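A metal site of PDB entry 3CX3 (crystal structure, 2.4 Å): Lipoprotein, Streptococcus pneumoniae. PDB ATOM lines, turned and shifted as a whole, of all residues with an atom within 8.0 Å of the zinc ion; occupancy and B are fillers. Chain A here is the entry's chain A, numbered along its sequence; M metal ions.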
ATOM      1  N   PHE A  17      -4.050  -4.875  17.150  1.00  0.00           N
ATOM      2  CA  PHE A  17      -5.011  -4.714  18.238  1.00  0.00           C
ATOM      3  C   PHE A  17      -5.206  -6.039  18.979  1.00  0.00           C
ATOM      4  O   PHE A  17      -4.477  -6.988  18.702  1.00  0.00           O
ATOM      5  CB  PHE A  17      -6.296  -4.025  17.727  1.00  0.00           C
ATOM      6  CG  PHE A  17      -7.292  -4.952  17.078  1.00  0.00           C
ATOM      7  CD1 PHE A  17      -6.952  -5.681  15.919  1.00  0.00           C
ATOM      8  CD2 PHE A  17      -8.584  -5.035  17.565  1.00  0.00           C
ATOM      9  CE1 PHE A  17      -7.895  -6.527  15.293  1.00  0.00           C
ATOM     10  CE2 PHE A  17      -9.513  -5.855  16.970  1.00  0.00           C
ATOM     11  CZ  PHE A  17      -9.163  -6.620  15.802  1.00  0.00           C
ATOM     12  N   ILE A  43      -9.890   0.333  16.498  1.00  0.00           N
ATOM     13  CA  ILE A  43      -9.271  -0.326  15.328  1.00  0.00           C
ATOM     14  C   ILE A  43      -9.823   0.077  13.963  1.00  0.00           C
ATOM     15  O   ILE A  43      -9.084   0.074  12.974  1.00  0.00           O
ATOM     16  CB  ILE A  43      -9.267  -1.899  15.473  1.00  0.00           C
ATOM     17  CG1 ILE A  43      -8.465  -2.570  14.356  1.00  0.00           C
ATOM     18  CG2 ILE A  43     -10.695  -2.485  15.495  1.00  0.00           C
ATOM     19  CD1 ILE A  43      -6.972  -2.331  14.397  1.00  0.00           C
ATOM     20  N   HIS A  44     -11.133   0.369  13.915  1.00  0.00           N
ATOM     21  CA  HIS A  44     -11.852   0.749  12.697  1.00  0.00           C
ATOM     22  C   HIS A  44     -11.444   2.131  12.140  1.00  0.00           C
ATOM     23  O   HIS A  44     -11.278   2.301  10.936  1.00  0.00           O
ATOM     24  CB  HIS A  44     -13.369   0.688  12.957  1.00  0.00           C
ATOM     25  CG  HIS A  44     -13.904  -0.713  13.136  1.00  0.00           C
ATOM     26  ND1 HIS A  44     -14.306  -1.504  12.078  1.00  0.00           N
ATOM     27  CD2 HIS A  44     -14.136  -1.440  14.250  1.00  0.00           C
ATOM     28  CE1 HIS A  44     -14.742  -2.660  12.531  1.00  0.00           C
ATOM     29  NE2 HIS A  44     -14.642  -2.660  13.837  1.00  0.00           N
ATOM     30  N   LEU A  69      -9.420  -4.539   7.308  1.00  0.00           N
ATOM     31  CA  LEU A  69      -9.579  -3.873   8.609  1.00  0.00           C
ATOM     32  C   LEU A  69      -8.482  -2.810   8.774  1.00  0.00           C
ATOM     33  O   LEU A  69      -8.708  -1.604   8.617  1.00  0.00           O
ATOM     34  CB  LEU A  69      -9.502  -4.906   9.741  1.00  0.00           C
ATOM     35  CG  LEU A  69     -10.433  -4.842  10.977  1.00  0.00           C
ATOM     36  CD1 LEU A  69      -9.678  -5.308  12.271  1.00  0.00           C
ATOM     37  CD2 LEU A  69     -11.163  -3.475  11.161  1.00  0.00           C
ATOM     38  N   ASP A 118     -17.053  -8.070   5.931  1.00  0.00           N
ATOM     39  CA  ASP A 118     -17.078  -8.099   7.382  1.00  0.00           C
ATOM     40  C   ASP A 118     -15.829  -8.804   7.917  1.00  0.00           C
ATOM     41  O   ASP A 118     -15.641  -9.999   7.690  1.00  0.00           O
ATOM     42  CB  ASP A 118     -18.371  -8.750   7.918  1.00  0.00           C
ATOM     43  CG  ASP A 118     -18.457  -8.696   9.452  1.00  0.00           C
ATOM     44  OD1 ASP A 118     -17.478  -8.367  10.109  1.00  0.00           O
ATOM     45  OD2 ASP A 118     -19.512  -9.011  10.024  1.00  0.00           O
ATOM     46  N   PRO A 119     -14.993  -8.062   8.661  1.00  0.00           N
ATOM     47  CA  PRO A 119     -13.723  -8.576   9.176  1.00  0.00           C
ATOM     48  C   PRO A 119     -13.807  -9.382  10.478  1.00  0.00           C
ATOM     49  O   PRO A 119     -12.772  -9.895  10.930  1.00  0.00           O
ATOM     50  CB  PRO A 119     -12.938  -7.292   9.460  1.00  0.00           C
ATOM     51  CG  PRO A 119     -13.987  -6.272   9.836  1.00  0.00           C
ATOM     52  CD  PRO A 119     -15.195  -6.638   9.021  1.00  0.00           C
ATOM     53  N   HIS A 120     -15.001  -9.482  11.055  1.00  0.00           N
ATOM     54  CA  HIS A 120     -15.183  -9.704  12.504  1.00  0.00           C
ATOM     55  C   HIS A 120     -15.159 -11.158  12.902  1.00  0.00           C
ATOM     56  O   HIS A 120     -15.747 -11.600  13.906  1.00  0.00           O
ATOM     57  CB  HIS A 120     -16.485  -9.112  12.964  1.00  0.00           C
ATOM     58  CG  HIS A 120     -16.427  -7.655  13.257  1.00  0.00           C
ATOM     59  ND1 HIS A 120     -16.924  -6.716  12.377  1.00  0.00           N
ATOM     60  CD2 HIS A 120     -15.992  -6.982  14.361  1.00  0.00           C
ATOM     61  CE1 HIS A 120     -16.779  -5.510  12.931  1.00  0.00           C
ATOM     62  NE2 HIS A 120     -16.216  -5.646  14.124  1.00  0.00           N
ATOM     63  N   TRP A 122     -12.865 -13.055  14.372  1.00  0.00           N
ATOM     64  CA  TRP A 122     -12.282 -13.543  15.604  1.00  0.00           C
ATOM     65  C   TRP A 122     -13.273 -13.987  16.685  1.00  0.00           C
ATOM     66  O   TRP A 122     -12.898 -14.690  17.614  1.00  0.00           O
ATOM     67  CB  TRP A 122     -11.297 -12.503  16.161  1.00  0.00           C
ATOM     68  CG  TRP A 122     -11.897 -11.165  16.502  1.00  0.00           C
ATOM     69  CD1 TRP A 122     -12.390 -10.787  17.696  1.00  0.00           C
ATOM     70  CD2 TRP A 122     -12.013 -10.015  15.634  1.00  0.00           C
ATOM     71  NE1 TRP A 122     -12.833  -9.482  17.652  1.00  0.00           N
ATOM     72  CE2 TRP A 122     -12.607  -8.976  16.402  1.00  0.00           C
ATOM     73  CE3 TRP A 122     -11.670  -9.760  14.299  1.00  0.00           C
ATOM     74  CZ2 TRP A 122     -12.870  -7.699  15.878  1.00  0.00           C
ATOM     75  CZ3 TRP A 122     -11.936  -8.491  13.757  1.00  0.00           C
ATOM     76  CH2 TRP A 122     -12.524  -7.472  14.555  1.00  0.00           C
ATOM     77  N   LEU A 123     -14.547 -13.589  16.519  1.00  0.00           N
ATOM     78  CA  LEU A 123     -15.625 -13.814  17.496  1.00  0.00           C
ATOM     79  C   LEU A 123     -16.332 -15.129  17.301  1.00  0.00           C
ATOM     80  O   LEU A 123     -17.205 -15.510  18.082  1.00  0.00           O
ATOM     81  CB  LEU A 123     -16.661 -12.687  17.393  1.00  0.00           C
ATOM     82  CG  LEU A 123     -16.211 -11.345  17.982  1.00  0.00           C
ATOM     83  CD1 LEU A 123     -17.306 -10.297  17.758  1.00  0.00           C
ATOM     84  CD2 LEU A 123     -15.826 -11.466  19.494  1.00  0.00           C
ATOM     85  N   HIS A 184     -22.265  -1.923  17.591  1.00  0.00           N
ATOM     86  CA  HIS A 184     -22.033  -1.969  16.141  1.00  0.00           C
ATOM     87  C   HIS A 184     -22.091  -3.378  15.573  1.00  0.00           C
ATOM     88  O   HIS A 184     -22.238  -4.335  16.321  1.00  0.00           O
ATOM     89  CB  HIS A 184     -20.792  -1.203  15.739  1.00  0.00           C
ATOM     90  CG  HIS A 184     -19.501  -1.938  15.928  1.00  0.00           C
ATOM     91  ND1 HIS A 184     -18.890  -2.072  17.166  1.00  0.00           N
ATOM     92  CD2 HIS A 184     -18.653  -2.500  15.033  1.00  0.00           C
ATOM     93  CE1 HIS A 184     -17.743  -2.713  17.018  1.00  0.00           C
ATOM     94  NE2 HIS A 184     -17.575  -2.991  15.734  1.00  0.00           N
ATOM     95  N   THR A 185     -22.005  -3.503  14.257  1.00  0.00           N
ATOM     96  CA  THR A 185     -22.162  -4.803  13.613  1.00  0.00           C
ATOM     97  C   THR A 185     -20.894  -5.653  13.768  1.00  0.00           C
ATOM     98  O   THR A 185     -20.092  -5.761  12.825  1.00  0.00           O
ATOM     99  CB  THR A 185     -22.528  -4.681  12.098  1.00  0.00           C
ATOM    100  OG1 THR A 185     -23.600  -3.752  11.922  1.00  0.00           O
ATOM    101  CG2 THR A 185     -22.924  -6.031  11.526  1.00  0.00           C
ATOM    102  N   ALA A 186     -20.733  -6.292  14.935  1.00  0.00           N
ATOM    103  CA  ALA A 186     -19.561  -7.092  15.183  1.00  0.00           C
ATOM    104  C   ALA A 186     -19.768  -8.602  15.300  1.00  0.00           C
ATOM    105  O   ALA A 186     -18.853  -9.376  15.082  1.00  0.00           O
ATOM    106  CB  ALA A 186     -18.817  -6.558  16.396  1.00  0.00           C
ATOM    107  N   PHE A 187     -20.981  -9.028  15.649  1.00  0.00           N
ATOM    108  CA  PHE A 187     -21.263 -10.389  16.066  1.00  0.00           C
ATOM    109  C   PHE A 187     -21.858 -11.265  14.989  1.00  0.00           C
ATOM    110  O   PHE A 187     -22.428 -12.320  15.275  1.00  0.00           O
ATOM    111  CB  PHE A 187     -22.140 -10.347  17.314  1.00  0.00           C
ATOM    112  CG  PHE A 187     -21.452  -9.667  18.472  1.00  0.00           C
ATOM    113  CD1 PHE A 187     -20.723 -10.414  19.385  1.00  0.00           C
ATOM    114  CD2 PHE A 187     -21.480  -8.287  18.603  1.00  0.00           C
ATOM    115  CE1 PHE A 187     -20.051  -9.790  20.439  1.00  0.00           C
ATOM    116  CE2 PHE A 187     -20.819  -7.667  19.649  1.00  0.00           C
ATOM    117  CZ  PHE A 187     -20.091  -8.427  20.557  1.00  0.00           C
ATOM    118  N   GLY A 203     -22.946   0.096  11.387  1.00  0.00           N
ATOM    119  CA  GLY A 203     -22.470  -0.898  10.419  1.00  0.00           C
ATOM    120  C   GLY A 203     -21.221  -1.630  10.889  1.00  0.00           C
ATOM    121  O   GLY A 203     -20.927  -1.666  12.081  1.00  0.00           O
ATOM    122  N   ILE A 204     -20.447  -2.197   9.975  1.00  0.00           N
ATOM    123  CA  ILE A 204     -19.284  -2.973  10.467  1.00  0.00           C
ATOM    124  C   ILE A 204     -18.311  -2.140  11.315  1.00  0.00           C
ATOM    125  O   ILE A 204     -17.657  -2.680  12.194  1.00  0.00           O
ATOM    126  CB  ILE A 204     -18.558  -3.854   9.388  1.00  0.00           C
ATOM    127  CG1 ILE A 204     -17.226  -3.244   8.952  1.00  0.00           C
ATOM    128  CG2 ILE A 204     -19.501  -4.232   8.239  1.00  0.00           C
ATOM    129  CD1 ILE A 204     -17.213  -2.605   7.558  1.00  0.00           C
ATOM    130  N   SER A 205     -18.225  -0.838  11.043  1.00  0.00           N
ATOM    131  CA  SER A 205     -17.423   0.072  11.862  1.00  0.00           C
ATOM    132  C   SER A 205     -18.322   1.015  12.666  1.00  0.00           C
ATOM    133  O   SER A 205     -19.388   1.412  12.180  1.00  0.00           O
ATOM    134  CB  SER A 205     -16.415   0.817  11.000  1.00  0.00           C
ATOM    135  OG  SER A 205     -16.598   2.206  11.064  1.00  0.00           O
ATOM    136  N   PRO A 206     -17.930   1.351  13.912  1.00  0.00           N
ATOM    137  CA  PRO A 206     -18.744   2.150  14.820  1.00  0.00           C
ATOM    138  C   PRO A 206     -19.071   3.542  14.300  1.00  0.00           C
ATOM    139  O   PRO A 206     -20.025   4.159  14.781  1.00  0.00           O
ATOM    140  CB  PRO A 206     -17.848   2.275  16.054  1.00  0.00           C
ATOM    141  CG  PRO A 206     -16.988   1.077  16.007  1.00  0.00           C
ATOM    142  CD  PRO A 206     -16.671   0.944  14.558  1.00  0.00           C
ATOM    143  N   GLU A 233     -21.158  -1.411  24.500  1.00  0.00           N
ATOM    144  CA  GLU A 233     -19.830  -1.613  25.068  1.00  0.00           C
ATOM    145  C   GLU A 233     -19.570  -0.544  26.126  1.00  0.00           C
ATOM    146  O   GLU A 233     -20.432   0.280  26.425  1.00  0.00           O
ATOM    147  CB  GLU A 233     -18.754  -1.517  23.993  1.00  0.00           C
ATOM    148  CG  GLU A 233     -19.036  -2.282  22.706  1.00  0.00           C
ATOM    149  CD  GLU A 233     -18.604  -1.484  21.473  1.00  0.00           C
ATOM    150  OE1 GLU A 233     -18.083  -0.366  21.663  1.00  0.00           O
ATOM    151  OE2 GLU A 233     -18.800  -1.964  20.324  1.00  0.00           O
ATOM    152  N   PRO A 257     -16.874  -6.906  21.879  1.00  0.00           N
ATOM    153  CA  PRO A 257     -16.468  -7.418  20.570  1.00  0.00           C
ATOM    154  C   PRO A 257     -14.941  -7.644  20.532  1.00  0.00           C
ATOM    155  O   PRO A 257     -14.387  -7.997  19.461  1.00  0.00           O
ATOM    156  CB  PRO A 257     -16.891  -6.302  19.623  1.00  0.00           C
ATOM    157  CG  PRO A 257     -16.861  -5.037  20.402  1.00  0.00           C
ATOM    158  CD  PRO A 257     -16.978  -5.430  21.893  1.00  0.00           C
ATOM    159  N   LEU A 258     -14.286  -7.449  21.686  1.00  0.00           N
ATOM    160  CA  LEU A 258     -12.848  -7.657  21.898  1.00  0.00           C
ATOM    161  C   LEU A 258     -11.913  -6.795  21.052  1.00  0.00           C
ATOM    162  O   LEU A 258     -10.756  -7.128  20.856  1.00  0.00           O
ATOM    163  CB  LEU A 258     -12.473  -9.134  21.808  1.00  0.00           C
ATOM    164  CG  LEU A 258     -13.355 -10.117  22.588  1.00  0.00           C
ATOM    165  CD1 LEU A 258     -13.089 -11.555  22.123  1.00  0.00           C
ATOM    166  CD2 LEU A 258     -13.213  -9.993  24.099  1.00  0.00           C
ATOM    167  N   GLU A 259     -12.411  -5.664  20.607  1.00  0.00           N
ATOM    168  CA  GLU A 259     -11.618  -4.720  19.836  1.00  0.00           C
ATOM    169  C   GLU A 259     -10.648  -3.929  20.714  1.00  0.00           C
ATOM    170  O   GLU A 259      -9.509  -3.664  20.315  1.00  0.00           O
ATOM    171  CB  GLU A 259     -12.544  -3.812  19.050  1.00  0.00           C
ATOM    172  CG  GLU A 259     -13.124  -4.480  17.814  1.00  0.00           C
ATOM    173  CD  GLU A 259     -14.355  -3.773  17.330  1.00  0.00           C
ATOM    174  OE1 GLU A 259     -14.414  -2.539  17.486  1.00  0.00           O
ATOM    175  OE2 GLU A 259     -15.271  -4.452  16.836  1.00  0.00           O
HETATM  176 ZN    ZN M   1     -15.845  -3.814  14.942  1.00  0.00          ZN
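NE2 of His 44 is bound to the zinc ion (2.0 Å).
NE2 of His 120 is bound to the zinc ion, 2.0 Å away.
NE2 of His 184 binds the zinc ion, at 2.1 Å.
The side-chain carboxylate (OE2) of Glu 259 binds the zinc ion (2.1 Å).
Merely in contact with the zinc ion: Ile 204 (3.5 Å).
Within 4 Å of the zinc ion: His 44, His 120, His 184, Ile 204 and Glu 259.
The nearest printed residue that does not touch the zinc ion is Ala 186 (4.3 Å).
ND1 of His 184 is in hydrogen-bond range of OE2 of Glu 233, at 3.2 Å.
A ring nitrogen (ND1) of His 120 lies close to the backbone carbonyl oxygen (O) of Thr 185, 3.3 Å away.
The side-chain carboxylate of Asp 118 lies within hydrogen-bond range of a ring nitrogen (ND1) of His 120.
A ring nitrogen (NE2) of His 44 sits close to the backbone carbonyl oxygen (O) of Ile 204, at 3.4 Å.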
